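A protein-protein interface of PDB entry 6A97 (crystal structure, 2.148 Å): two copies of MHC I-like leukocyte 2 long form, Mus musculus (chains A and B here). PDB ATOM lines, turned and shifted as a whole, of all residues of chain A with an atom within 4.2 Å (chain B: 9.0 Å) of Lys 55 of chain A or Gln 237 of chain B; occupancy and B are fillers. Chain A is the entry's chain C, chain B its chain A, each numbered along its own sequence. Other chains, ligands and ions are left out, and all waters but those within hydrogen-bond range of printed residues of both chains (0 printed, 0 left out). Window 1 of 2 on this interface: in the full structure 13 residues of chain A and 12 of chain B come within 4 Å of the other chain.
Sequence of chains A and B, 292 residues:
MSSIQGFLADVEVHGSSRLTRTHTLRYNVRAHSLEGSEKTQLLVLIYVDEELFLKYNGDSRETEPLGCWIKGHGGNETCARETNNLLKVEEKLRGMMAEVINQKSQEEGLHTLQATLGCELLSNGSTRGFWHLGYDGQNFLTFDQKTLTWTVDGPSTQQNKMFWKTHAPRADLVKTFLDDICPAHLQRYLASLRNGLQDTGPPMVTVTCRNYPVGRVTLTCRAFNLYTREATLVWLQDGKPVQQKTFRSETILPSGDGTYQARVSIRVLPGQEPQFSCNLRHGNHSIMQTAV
O of Pro 241 of chain B is in hydrogen-bond range of NE1 of Trp 69 of chain A (3.4 Å).
The side-chain amino group (NZ) of Lys 55 of chain A sits at hydrogen-bond distance from the side-chain amide oxygen (OE1) of Gln 237 of chain B.
The backbone carbonyl oxygen (O) of Trp 235 of chain B is in hydrogen-bond range of the backbone NH (N) of Val 242 of chain B (2.8 Å).
The side-chain amide nitrogen (NE2) of Gln 237 of chain B lies within hydrogen-bond range of the side-chain amide oxygen (OE1) of Gln 275 of chain B, at 3.0 Å.
O of Lys 55 of chain A lies within hydrogen-bond range of N of Gly 67 of chain A, at 2.8 Å.
Among the printed residues, merely in contact across the chains: Trp 69 of chain A with Lys 240 of chain B (3.3 Å), Leu 52 of chain A with Gln 237 of chain B (3.4 Å), Leu 45 of chain A with Gln 237 of chain B (3.7 Å), Lys 55 of chain A with Val 242 of chain B (3.7 Å) and Leu 52 of chain A with Lys 240 of chain B (3.7 Å).
Lys 55 of chain A touches just these residues of chain B: Gln 237 (3.0 Å) and Val 242 (3.7 Å).
Gln 237 of chain B touches just these residues of chain A: Leu 45, Leu 52 and Lys 55.
No residue of chain B comes within 4 Å of Gly 67 of chain A.
Of the printed residues of chain A, Val 242 of chain B touches Lys 55 (3.7 Å).
Printed residues of chain B within 4 Å of Leu 45 of chain A: Gln 237 (3.7 Å).
Of the printed residues of chain A, Pro 241 of chain B touches Trp 69 (3.4 Å).
The nearest residue of chain B that does not touch Lys 55 of chain A is Phe 276 of chain B (4.9 Å).
Of the 24 printed residues of chain B, 4 touch a printed residue of chain A.
Of the 12 printed residues of chain A, 4 touch a printed residue of chain B.
Hydrophobic or aromatic side chains of chain A within 4 Å of the printed part of chain B: Leu 45, Leu 52 and Trp 69.
Among the printed residues, 7 pairs touch across the chains.
Among the printed residues, no Asp or Glu carboxylate lies within 4 Å of a Lys or Arg side-chain nitrogen of the other chain.
No position is printed for both chains.
Of the 7 pairs that touch across the chains among the printed residues, none has its exchanged pair printed and touching as well.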
ATOM      1  N   VAL A  44      20.569 -36.016 -31.145  1.00  0.00           N
ATOM      2  CA  VAL A  44      19.512 -35.515 -32.012  1.00  0.00           C
ATOM      3  C   VAL A  44      18.596 -34.553 -31.273  1.00  0.00           C
ATOM      4  O   VAL A  44      18.290 -34.721 -30.090  1.00  0.00           O
ATOM      5  CB  VAL A  44      18.682 -36.670 -32.653  1.00  0.00           C
ATOM      6  CG1 VAL A  44      19.416 -38.000 -32.534  1.00  0.00           C
ATOM      7  CG2 VAL A  44      17.282 -36.758 -32.063  1.00  0.00           C
ATOM      8  N   LEU A  45      18.212 -33.504 -31.988  1.00  0.00           N
ATOM      9  CA  LEU A  45      17.237 -32.546 -31.508  1.00  0.00           C
ATOM     10  C   LEU A  45      16.092 -32.537 -32.503  1.00  0.00           C
ATOM     11  O   LEU A  45      16.309 -32.457 -33.718  1.00  0.00           O
ATOM     12  CB  LEU A  45      17.854 -31.156 -31.366  1.00  0.00           C
ATOM     13  CG  LEU A  45      19.031 -31.045 -30.395  1.00  0.00           C
ATOM     14  CD1 LEU A  45      19.792 -29.747 -30.607  1.00  0.00           C
ATOM     15  CD2 LEU A  45      18.526 -31.132 -28.978  1.00  0.00           C
ATOM     16  N   LEU A  52      11.623 -26.773 -29.680  1.00  0.00           N
ATOM     17  CA  LEU A  52      12.308 -27.978 -29.226  1.00  0.00           C
ATOM     18  C   LEU A  52      11.326 -28.925 -28.546  1.00  0.00           C
ATOM     19  O   LEU A  52      10.602 -28.541 -27.629  1.00  0.00           O
ATOM     20  CB  LEU A  52      13.459 -27.619 -28.286  1.00  0.00           C
ATOM     21  CG  LEU A  52      14.387 -28.762 -27.872  1.00  0.00           C
ATOM     22  CD1 LEU A  52      15.016 -29.418 -29.099  1.00  0.00           C
ATOM     23  CD2 LEU A  52      15.461 -28.245 -26.929  1.00  0.00           C
ATOM     24  N   LEU A  54      11.768 -33.011 -28.783  1.00  0.00           N
ATOM     25  CA  LEU A  54      12.448 -34.202 -28.278  1.00  0.00           C
ATOM     26  C   LEU A  54      13.960 -34.024 -28.334  1.00  0.00           C
ATOM     27  O   LEU A  54      14.480 -33.314 -29.198  1.00  0.00           O
ATOM     28  CB  LEU A  54      12.045 -35.445 -29.071  1.00  0.00           C
ATOM     29  CG  LEU A  54      10.684 -36.077 -28.777  1.00  0.00           C
ATOM     30  CD1 LEU A  54      10.338 -37.128 -29.824  1.00  0.00           C
ATOM     31  CD2 LEU A  54      10.668 -36.682 -27.383  1.00  0.00           C
ATOM     32  N   LYS A  55      14.662 -34.673 -27.413  1.00  0.00           N
ATOM     33  CA  LYS A  55      16.117 -34.614 -27.386  1.00  0.00           C
ATOM     34  C   LYS A  55      16.724 -35.928 -26.918  1.00  0.00           C
ATOM     35  O   LYS A  55      16.344 -36.460 -25.880  1.00  0.00           O
ATOM     36  CB  LYS A  55      16.594 -33.478 -26.483  1.00  0.00           C
ATOM     37  CG  LYS A  55      18.102 -33.441 -26.287  1.00  0.00           C
ATOM     38  CD  LYS A  55      18.517 -32.296 -25.379  1.00  0.00           C
ATOM     39  CE  LYS A  55      20.027 -32.270 -25.171  1.00  0.00           C
ATOM     40  NZ  LYS A  55      20.435 -31.183 -24.234  1.00  0.00           N
ATOM     41  N   TYR A  56      17.666 -36.451 -27.696  1.00  0.00           N
ATOM     42  CA  TYR A  56      18.421 -37.617 -27.266  1.00  0.00           C
ATOM     43  C   TYR A  56      19.910 -37.320 -27.234  1.00  0.00           C
ATOM     44  O   TYR A  56      20.530 -37.075 -28.271  1.00  0.00           O
ATOM     45  CB  TYR A  56      18.156 -38.823 -28.169  1.00  0.00           C
ATOM     46  CG  TYR A  56      18.971 -40.029 -27.758  1.00  0.00           C
ATOM     47  CD1 TYR A  56      19.040 -40.421 -26.425  1.00  0.00           C
ATOM     48  CD2 TYR A  56      19.678 -40.772 -28.695  1.00  0.00           C
ATOM     49  CE1 TYR A  56      19.786 -41.514 -26.037  1.00  0.00           C
ATOM     50  CE2 TYR A  56      20.426 -41.873 -28.317  1.00  0.00           C
ATOM     51  CZ  TYR A  56      20.477 -42.239 -26.987  1.00  0.00           C
ATOM     52  OH  TYR A  56      21.220 -43.333 -26.604  1.00  0.00           O
ATOM     53  N   ASN A  57      20.468 -37.356 -26.027  1.00  0.00           N
ATOM     54  CA  ASN A  57      21.891 -37.148 -25.796  1.00  0.00           C
ATOM     55  C   ASN A  57      22.488 -38.357 -25.082  1.00  0.00           C
ATOM     56  O   ASN A  57      22.486 -38.423 -23.854  1.00  0.00           O
ATOM     57  CB  ASN A  57      22.116 -35.871 -24.975  1.00  0.00           C
ATOM     58  CG  ASN A  57      23.584 -35.627 -24.651  1.00  0.00           C
ATOM     59  OD1 ASN A  57      24.480 -36.242 -25.232  1.00  0.00           O
ATOM     60  ND2 ASN A  57      23.833 -34.722 -23.710  1.00  0.00           N
ATOM     61  N   PRO A  65      19.531 -38.029 -20.515  1.00  0.00           N
ATOM     62  CA  PRO A  65      19.805 -38.468 -21.890  1.00  0.00           C
ATOM     63  C   PRO A  65      18.571 -38.343 -22.774  1.00  0.00           C
ATOM     64  O   PRO A  65      18.683 -38.079 -23.973  1.00  0.00           O
ATOM     65  CB  PRO A  65      20.218 -39.935 -21.724  1.00  0.00           C
ATOM     66  CG  PRO A  65      19.667 -40.345 -20.394  1.00  0.00           C
ATOM     67  CD  PRO A  65      19.688 -39.119 -19.536  1.00  0.00           C
ATOM     68  N   LEU A  66      17.400 -38.533 -22.181  1.00  0.00           N
ATOM     69  CA  LEU A  66      16.149 -38.399 -22.911  1.00  0.00           C
ATOM     70  C   LEU A  66      15.398 -37.168 -22.433  1.00  0.00           C
ATOM     71  O   LEU A  66      15.031 -37.064 -21.263  1.00  0.00           O
ATOM     72  CB  LEU A  66      15.291 -39.652 -22.747  1.00  0.00           C
ATOM     73  CG  LEU A  66      15.883 -40.903 -23.395  1.00  0.00           C
ATOM     74  CD1 LEU A  66      15.266 -42.172 -22.818  1.00  0.00           C
ATOM     75  CD2 LEU A  66      15.691 -40.844 -24.899  1.00  0.00           C
ATOM     76  N   GLY A  67      15.189 -36.227 -23.346  1.00  0.00           N
ATOM     77  CA  GLY A  67      14.512 -34.990 -23.019  1.00  0.00           C
ATOM     78  C   GLY A  67      13.220 -34.847 -23.792  1.00  0.00           C
ATOM     79  O   GLY A  67      13.160 -35.145 -24.984  1.00  0.00           O
ATOM     80  N   TRP A  69       9.560 -32.168 -23.773  1.00  0.00           N
ATOM     81  CA  TRP A  69       8.827 -31.053 -23.198  1.00  0.00           C
ATOM     82  C   TRP A  69       7.453 -30.914 -23.843  1.00  0.00           C
ATOM     83  O   TRP A  69       7.344 -30.693 -25.050  1.00  0.00           O
ATOM     84  CB  TRP A  69       9.623 -29.760 -23.362  1.00  0.00           C
ATOM     85  CG  TRP A  69      11.028 -29.853 -22.857  1.00  0.00           C
ATOM     86  CD1 TRP A  69      11.496 -29.420 -21.651  1.00  0.00           C
ATOM     87  CD2 TRP A  69      12.154 -30.409 -23.548  1.00  0.00           C
ATOM     88  NE1 TRP A  69      12.844 -29.672 -21.548  1.00  0.00           N
ATOM     89  CE2 TRP A  69      13.270 -30.280 -22.701  1.00  0.00           C
ATOM     90  CE3 TRP A  69      12.324 -31.003 -24.803  1.00  0.00           C
ATOM     91  CZ2 TRP A  69      14.539 -30.724 -23.064  1.00  0.00           C
ATOM     92  CZ3 TRP A  69      13.584 -31.444 -25.162  1.00  0.00           C
ATOM     93  CH2 TRP A  69      14.674 -31.304 -24.296  1.00  0.00           C
ATOM     94  N   LEU A  86      12.188 -42.422 -30.356  1.00  0.00           N
ATOM     95  CA  LEU A  86      13.335 -41.531 -30.498  1.00  0.00           C
ATOM     96  C   LEU A  86      14.637 -42.313 -30.632  1.00  0.00           C
ATOM     97  O   LEU A  86      15.458 -42.021 -31.502  1.00  0.00           O
ATOM     98  CB  LEU A  86      13.415 -40.573 -29.310  1.00  0.00           C
ATOM     99  CG  LEU A  86      14.583 -39.590 -29.321  1.00  0.00           C
ATOM    100  CD1 LEU A  86      14.587 -38.799 -30.610  1.00  0.00           C
ATOM    101  CD2 LEU A  86      14.508 -38.656 -28.129  1.00  0.00           C
ATOM    102  N   LEU B 219      30.331 -25.492 -20.102  1.00  0.00           N
ATOM    103  CA  LEU B 219      29.755 -24.188 -19.798  1.00  0.00           C
ATOM    104  C   LEU B 219      29.482 -24.098 -18.309  1.00  0.00           C
ATOM    105  O   LEU B 219      28.779 -24.941 -17.755  1.00  0.00           O
ATOM    106  CB  LEU B 219      28.461 -23.959 -20.582  1.00  0.00           C
ATOM    107  CG  LEU B 219      28.549 -24.027 -22.109  1.00  0.00           C
ATOM    108  CD1 LEU B 219      27.161 -23.903 -22.738  1.00  0.00           C
ATOM    109  CD2 LEU B 219      29.469 -22.952 -22.637  1.00  0.00           C
ATOM    110  N   VAL B 234      19.198 -22.501 -13.735  1.00  0.00           N
ATOM    111  CA  VAL B 234      18.765 -23.439 -14.759  1.00  0.00           C
ATOM    112  C   VAL B 234      19.486 -23.142 -16.068  1.00  0.00           C
ATOM    113  O   VAL B 234      19.611 -21.986 -16.470  1.00  0.00           O
ATOM    114  CB  VAL B 234      17.228 -23.392 -14.972  1.00  0.00           C
ATOM    115  CG1 VAL B 234      16.752 -21.974 -15.211  1.00  0.00           C
ATOM    116  CG2 VAL B 234      16.814 -24.297 -16.125  1.00  0.00           C
ATOM    117  N   TRP B 235      20.004 -24.186 -16.704  1.00  0.00           N
ATOM    118  CA  TRP B 235      20.524 -24.068 -18.055  1.00  0.00           C
ATOM    119  C   TRP B 235      19.384 -24.310 -19.030  1.00  0.00           C
ATOM    120  O   TRP B 235      18.641 -25.285 -18.899  1.00  0.00           O
ATOM    121  CB  TRP B 235      21.665 -25.056 -18.299  1.00  0.00           C
ATOM    122  CG  TRP B 235      23.010 -24.520 -17.927  1.00  0.00           C
ATOM    123  CD1 TRP B 235      23.775 -24.887 -16.855  1.00  0.00           C
ATOM    124  CD2 TRP B 235      23.749 -23.505 -18.619  1.00  0.00           C
ATOM    125  NE1 TRP B 235      24.946 -24.172 -16.844  1.00  0.00           N
ATOM    126  CE2 TRP B 235      24.954 -23.315 -17.916  1.00  0.00           C
ATOM    127  CE3 TRP B 235      23.506 -22.737 -19.762  1.00  0.00           C
ATOM    128  CZ2 TRP B 235      25.914 -22.392 -18.318  1.00  0.00           C
ATOM    129  CZ3 TRP B 235      24.463 -21.820 -20.161  1.00  0.00           C
ATOM    130  CH2 TRP B 235      25.651 -21.657 -19.444  1.00  0.00           C
ATOM    131  N   LEU B 236      19.247 -23.414 -20.003  1.00  0.00           N
ATOM    132  CA  LEU B 236      18.156 -23.482 -20.965  1.00  0.00           C
ATOM    133  C   LEU B 236      18.686 -23.694 -22.375  1.00  0.00           C
ATOM    134  O   LEU B 236      19.621 -23.020 -22.799  1.00  0.00           O
ATOM    135  CB  LEU B 236      17.313 -22.202 -20.915  1.00  0.00           C
ATOM    136  CG  LEU B 236      16.606 -21.881 -19.592  1.00  0.00           C
ATOM    137  CD1 LEU B 236      16.120 -20.439 -19.583  1.00  0.00           C
ATOM    138  CD2 LEU B 236      15.451 -22.825 -19.362  1.00  0.00           C
ATOM    139  N   GLN B 237      18.093 -24.639 -23.094  1.00  0.00           N
ATOM    140  CA  GLN B 237      18.395 -24.814 -24.506  1.00  0.00           C
ATOM    141  C   GLN B 237      17.124 -24.596 -25.306  1.00  0.00           C
ATOM    142  O   GLN B 237      16.167 -25.362 -25.175  1.00  0.00           O
ATOM    143  CB  GLN B 237      18.974 -26.200 -24.789  1.00  0.00           C
ATOM    144  CG  GLN B 237      19.109 -26.488 -26.277  1.00  0.00           C
ATOM    145  CD  GLN B 237      19.922 -27.733 -26.571  1.00  0.00           C
ATOM    146  OE1 GLN B 237      19.900 -28.699 -25.810  1.00  0.00           O
ATOM    147  NE2 GLN B 237      20.646 -27.716 -27.685  1.00  0.00           N
ATOM    148  N   ASP B 238      17.123 -23.548 -26.125  1.00  0.00           N
ATOM    149  CA  ASP B 238      15.934 -23.132 -26.865  1.00  0.00           C
ATOM    150  C   ASP B 238      14.723 -23.021 -25.939  1.00  0.00           C
ATOM    151  O   ASP B 238      13.661 -23.572 -26.222  1.00  0.00           O
ATOM    152  CB  ASP B 238      15.642 -24.103 -28.012  1.00  0.00           C
ATOM    153  CG  ASP B 238      16.801 -24.219 -28.983  1.00  0.00           C
ATOM    154  OD1 ASP B 238      17.427 -23.182 -29.289  1.00  0.00           O
ATOM    155  OD2 ASP B 238      17.086 -25.347 -29.439  1.00  0.00           O
ATOM    156  N   GLY B 239      14.904 -22.326 -24.819  1.00  0.00           N
ATOM    157  CA  GLY B 239      13.827 -22.084 -23.876  1.00  0.00           C
ATOM    158  C   GLY B 239      13.480 -23.263 -22.988  1.00  0.00           C
ATOM    159  O   GLY B 239      12.611 -23.157 -22.121  1.00  0.00           O
ATOM    160  N   LYS B 240      14.156 -24.389 -23.195  1.00  0.00           N
ATOM    161  CA  LYS B 240      13.842 -25.607 -22.454  1.00  0.00           C
ATOM    162  C   LYS B 240      14.946 -25.957 -21.461  1.00  0.00           C
ATOM    163  O   LYS B 240      16.121 -25.950 -21.814  1.00  0.00           O
ATOM    164  CB  LYS B 240      13.609 -26.774 -23.417  1.00  0.00           C
ATOM    165  CG  LYS B 240      12.170 -26.912 -23.911  1.00  0.00           C
ATOM    166  CD  LYS B 240      11.690 -25.692 -24.680  1.00  0.00           C
ATOM    167  CE  LYS B 240      10.244 -25.858 -25.123  1.00  0.00           C
ATOM    168  NZ  LYS B 240       9.736 -24.642 -25.818  1.00  0.00           N
ATOM    169  N   PRO B 241      14.566 -26.272 -20.215  1.00  0.00           N
ATOM    170  CA  PRO B 241      15.545 -26.591 -19.170  1.00  0.00           C
ATOM    171  C   PRO B 241      16.269 -27.904 -19.445  1.00  0.00           C
ATOM    172  O   PRO B 241      15.631 -28.936 -19.664  1.00  0.00           O
ATOM    173  CB  PRO B 241      14.691 -26.689 -17.899  1.00  0.00           C
ATOM    174  CG  PRO B 241      13.321 -26.998 -18.380  1.00  0.00           C
ATOM    175  CD  PRO B 241      13.180 -26.335 -19.720  1.00  0.00           C
ATOM    176  N   VAL B 242      17.597 -27.862 -19.447  1.00  0.00           N
ATOM    177  CA  VAL B 242      18.387 -29.062 -19.686  1.00  0.00           C
ATOM    178  C   VAL B 242      19.128 -29.468 -18.419  1.00  0.00           C
ATOM    179  O   VAL B 242      19.499 -30.629 -18.247  1.00  0.00           O
ATOM    180  CB  VAL B 242      19.388 -28.866 -20.840  1.00  0.00           C
ATOM    181  CG1 VAL B 242      18.647 -28.744 -22.158  1.00  0.00           C
ATOM    182  CG2 VAL B 242      20.257 -27.644 -20.596  1.00  0.00           C
ATOM    183  N   GLN B 243      19.337 -28.501 -17.535  1.00  0.00           N
ATOM    184  CA  GLN B 243      19.862 -28.768 -16.203  1.00  0.00           C
ATOM    185  C   GLN B 243      19.309 -27.719 -15.253  1.00  0.00           C
ATOM    186  O   GLN B 243      19.263 -26.533 -15.582  1.00  0.00           O
ATOM    187  CB  GLN B 243      21.393 -28.761 -16.190  1.00  0.00           C
ATOM    188  CG  GLN B 243      22.016 -29.063 -14.827  1.00  0.00           C
ATOM    189  CD  GLN B 243      21.645 -30.443 -14.295  1.00  0.00           C
ATOM    190  OE1 GLN B 243      20.588 -30.628 -13.687  1.00  0.00           O
ATOM    191  NE2 GLN B 243      22.517 -31.417 -14.524  1.00  0.00           N
ATOM    192  N   ILE B 266      27.399 -27.603 -17.459  1.00  0.00           N
ATOM    193  CA  ILE B 266      26.956 -28.600 -18.429  1.00  0.00           C
ATOM    194  C   ILE B 266      28.034 -28.784 -19.482  1.00  0.00           C
ATOM    195  O   ILE B 266      28.897 -27.921 -19.650  1.00  0.00           O
ATOM    196  CB  ILE B 266      25.639 -28.201 -19.134  1.00  0.00           C
ATOM    197  CG1 ILE B 266      25.789 -26.832 -19.802  1.00  0.00           C
ATOM    198  CG2 ILE B 266      24.471 -28.198 -18.146  1.00  0.00           C
ATOM    199  CD1 ILE B 266      24.580 -26.404 -20.608  1.00  0.00           C
ATOM    200  N   ARG B 267      27.982 -29.905 -20.193  1.00  0.00           N
ATOM    201  CA  ARG B 267      28.902 -30.143 -21.293  1.00  0.00           C
ATOM    202  C   ARG B 267      28.138 -30.155 -22.604  1.00  0.00           C
ATOM    203  O   ARG B 267      27.114 -30.824 -22.733  1.00  0.00           O
ATOM    204  CB  ARG B 267      29.662 -31.456 -21.097  1.00  0.00           C
ATOM    205  CG  ARG B 267      30.649 -31.405 -19.946  1.00  0.00           C
ATOM    206  CD  ARG B 267      30.539 -32.632 -19.071  1.00  0.00           C
ATOM    207  NE  ARG B 267      30.618 -32.280 -17.657  1.00  0.00           N
ATOM    208  CZ  ARG B 267      29.585 -31.847 -16.939  1.00  0.00           C
ATOM    209  NH1 ARG B 267      28.393 -31.715 -17.502  1.00  0.00           N
ATOM    210  NH2 ARG B 267      29.744 -31.547 -15.660  1.00  0.00           N
ATOM    211  N   VAL B 268      28.628 -29.385 -23.570  1.00  0.00           N
ATOM    212  CA  VAL B 268      28.005 -29.315 -24.878  1.00  0.00           C
ATOM    213  C   VAL B 268      29.066 -29.557 -25.928  1.00  0.00           C
ATOM    214  O   VAL B 268      30.253 -29.635 -25.608  1.00  0.00           O
ATOM    215  CB  VAL B 268      27.327 -27.951 -25.119  1.00  0.00           C
ATOM    216  CG1 VAL B 268      26.405 -27.618 -23.965  1.00  0.00           C
ATOM    217  CG2 VAL B 268      28.373 -26.855 -25.299  1.00  0.00           C
ATOM    218  N   LEU B 269      28.636 -29.686 -27.178  1.00  0.00           N
ATOM    219  CA  LEU B 269      29.556 -29.862 -28.290  1.00  0.00           C
ATOM    220  C   LEU B 269      30.069 -28.510 -28.777  1.00  0.00           C
ATOM    221  O   LEU B 269      29.358 -27.508 -28.688  1.00  0.00           O
ATOM    222  CB  LEU B 269      28.873 -30.617 -29.433  1.00  0.00           C
ATOM    223  CG  LEU B 269      28.259 -31.967 -29.063  1.00  0.00           C
ATOM    224  CD1 LEU B 269      27.510 -32.554 -30.249  1.00  0.00           C
ATOM    225  CD2 LEU B 269      29.334 -32.928 -28.568  1.00  0.00           C
ATOM    226  N   GLN B 272      28.127 -25.109 -30.064  1.00  0.00           N
ATOM    227  CA  GLN B 272      26.748 -25.115 -29.585  1.00  0.00           C
ATOM    228  C   GLN B 272      26.459 -24.021 -28.562  1.00  0.00           C
ATOM    229  O   GLN B 272      25.300 -23.791 -28.218  1.00  0.00           O
ATOM    230  CB  GLN B 272      26.396 -26.467 -28.965  1.00  0.00           C
ATOM    231  CG  GLN B 272      25.994 -27.546 -29.953  1.00  0.00           C
ATOM    232  CD  GLN B 272      25.361 -28.739 -29.260  1.00  0.00           C
ATOM    233  OE1 GLN B 272      25.814 -29.167 -28.194  1.00  0.00           O
ATOM    234  NE2 GLN B 272      24.298 -29.275 -29.855  1.00  0.00           N
ATOM    235  N   GLU B 273      27.509 -23.359 -28.074  1.00  0.00           N
ATOM    236  CA  GLU B 273      27.383 -22.406 -26.964  1.00  0.00           C
ATOM    237  C   GLU B 273      26.262 -21.362 -27.115  1.00  0.00           C
ATOM    238  O   GLU B 273      25.538 -21.121 -26.152  1.00  0.00           O
ATOM    239  CB  GLU B 273      28.717 -21.686 -26.726  1.00  0.00           C
ATOM    240  CG  GLU B 273      29.884 -22.606 -26.404  1.00  0.00           C
ATOM    241  CD  GLU B 273      30.699 -22.963 -27.632  1.00  0.00           C
ATOM    242  OE1 GLU B 273      30.094 -23.167 -28.705  1.00  0.00           O
ATOM    243  OE2 GLU B 273      31.942 -23.037 -27.525  1.00  0.00           O
ATOM    244  N   PRO B 274      26.111 -20.739 -28.307  1.00  0.00           N
ATOM    245  CA  PRO B 274      25.014 -19.767 -28.462  1.00  0.00           C
ATOM    246  C   PRO B 274      23.617 -20.299 -28.133  1.00  0.00           C
ATOM    247  O   PRO B 274      22.738 -19.504 -27.804  1.00  0.00           O
ATOM    248  CB  PRO B 274      25.094 -19.392 -29.945  1.00  0.00           C
ATOM    249  CG  PRO B 274      26.526 -19.541 -30.278  1.00  0.00           C
ATOM    250  CD  PRO B 274      27.011 -20.718 -29.479  1.00  0.00           C
ATOM    251  N   GLN B 275      23.416 -21.610 -28.212  1.00  0.00           N
ATOM    252  CA  GLN B 275      22.105 -22.196 -27.948  1.00  0.00           C
ATOM    253  C   GLN B 275      21.734 -22.199 -26.468  1.00  0.00           C
ATOM    254  O   GLN B 275      20.576 -22.418 -26.117  1.00  0.00           O
ATOM    255  CB  GLN B 275      22.048 -23.633 -28.472  1.00  0.00           C
ATOM    256  CG  GLN B 275      22.295 -23.777 -29.961  1.00  0.00           C
ATOM    257  CD  GLN B 275      22.243 -25.223 -30.412  1.00  0.00           C
ATOM    258  OE1 GLN B 275      21.389 -25.994 -29.969  1.00  0.00           O
ATOM    259  NE2 GLN B 275      23.159 -25.601 -31.294  1.00  0.00           N
ATOM    260  N   PHE B 276      22.711 -21.959 -25.598  1.00  0.00           N
ATOM    261  CA  PHE B 276      22.499 -22.165 -24.167  1.00  0.00           C
ATOM    262  C   PHE B 276      22.521 -20.872 -23.355  1.00  0.00           C
ATOM    263  O   PHE B 276      23.411 -20.038 -23.512  1.00  0.00           O
ATOM    264  CB  PHE B 276      23.548 -23.142 -23.626  1.00  0.00           C
ATOM    265  CG  PHE B 276      23.395 -24.542 -24.155  1.00  0.00           C
ATOM    266  CD1 PHE B 276      23.974 -24.906 -25.359  1.00  0.00           C
ATOM    267  CD2 PHE B 276      22.662 -25.487 -23.455  1.00  0.00           C
ATOM    268  CE1 PHE B 276      23.828 -26.187 -25.855  1.00  0.00           C
ATOM    269  CE2 PHE B 276      22.516 -26.773 -23.944  1.00  0.00           C
ATOM    270  CZ  PHE B 276      23.098 -27.122 -25.148  1.00  0.00           C
ATOM    271  N   SER B 277      21.531 -20.721 -22.484  1.00  0.00           N
ATOM    272  CA  SER B 277      21.453 -19.567 -21.596  1.00  0.00           C
ATOM    273  C   SER B 277      21.269 -20.030 -20.159  1.00  0.00           C
ATOM    274  O   SER B 277      20.604 -21.033 -19.907  1.00  0.00           O
ATOM    275  CB  SER B 277      20.303 -18.644 -22.003  1.00  0.00           C
ATOM    276  OG  SER B 277      20.414 -18.268 -23.364  1.00  0.00           O
ATOM    277  N   CYS B 278      21.865 -19.297 -19.224  1.00  0.00           N
ATOM    278  CA  CYS B 278      21.704 -19.580 -17.800  1.00  0.00           C
ATOM    279  C   CYS B 278      20.757 -18.579 -17.155  1.00  0.00           C
ATOM    280  O   CYS B 278      20.908 -17.375 -17.334  1.00  0.00           O
ATOM    281  CB  CYS B 278      23.055 -19.547 -17.085  1.00  0.00           C
ATOM    282  SG  CYS B 278      22.950 -19.985 -15.336  1.00  0.00           S
ATOM    283  N   ASN B 279      19.791 -19.074 -16.391  1.00  0.00           N
ATOM    284  CA  ASN B 279      18.810 -18.198 -15.761  1.00  0.00           C
ATOM    285  C   ASN B 279      18.828 -18.335 -14.243  1.00  0.00           C
ATOM    286  O   ASN B 279      18.585 -19.417 -13.698  1.00  0.00           O
ATOM    287  CB  ASN B 279      17.412 -18.493 -16.309  1.00  0.00           C
ATOM    288  CG  ASN B 279      16.356 -17.538 -15.777  1.00  0.00           C
ATOM    289  OD1 ASN B 279      15.164 -17.866 -15.756  1.00  0.00           O
ATOM    290  ND2 ASN B 279      16.781 -16.350 -15.349  1.00  0.00           N
ATOM    291  N   MET B 288      19.159 -13.502 -16.715  1.00  0.00           N
ATOM    292  CA  MET B 288      19.577 -14.495 -17.698  1.00  0.00           C
ATOM    293  C   MET B 288      20.814 -14.050 -18.463  1.00  0.00           C
ATOM    294  O   MET B 288      20.925 -12.893 -18.869  1.00  0.00           O
ATOM    295  CB  MET B 288      18.442 -14.797 -18.677  1.00  0.00           C
ATOM    296  CG  MET B 288      18.732 -15.973 -19.594  1.00  0.00           C
ATOM    297  SD  MET B 288      17.243 -16.861 -20.072  1.00  0.00           S
ATOM    298  CE  MET B 288      16.389 -15.613 -21.030  1.00  0.00           C
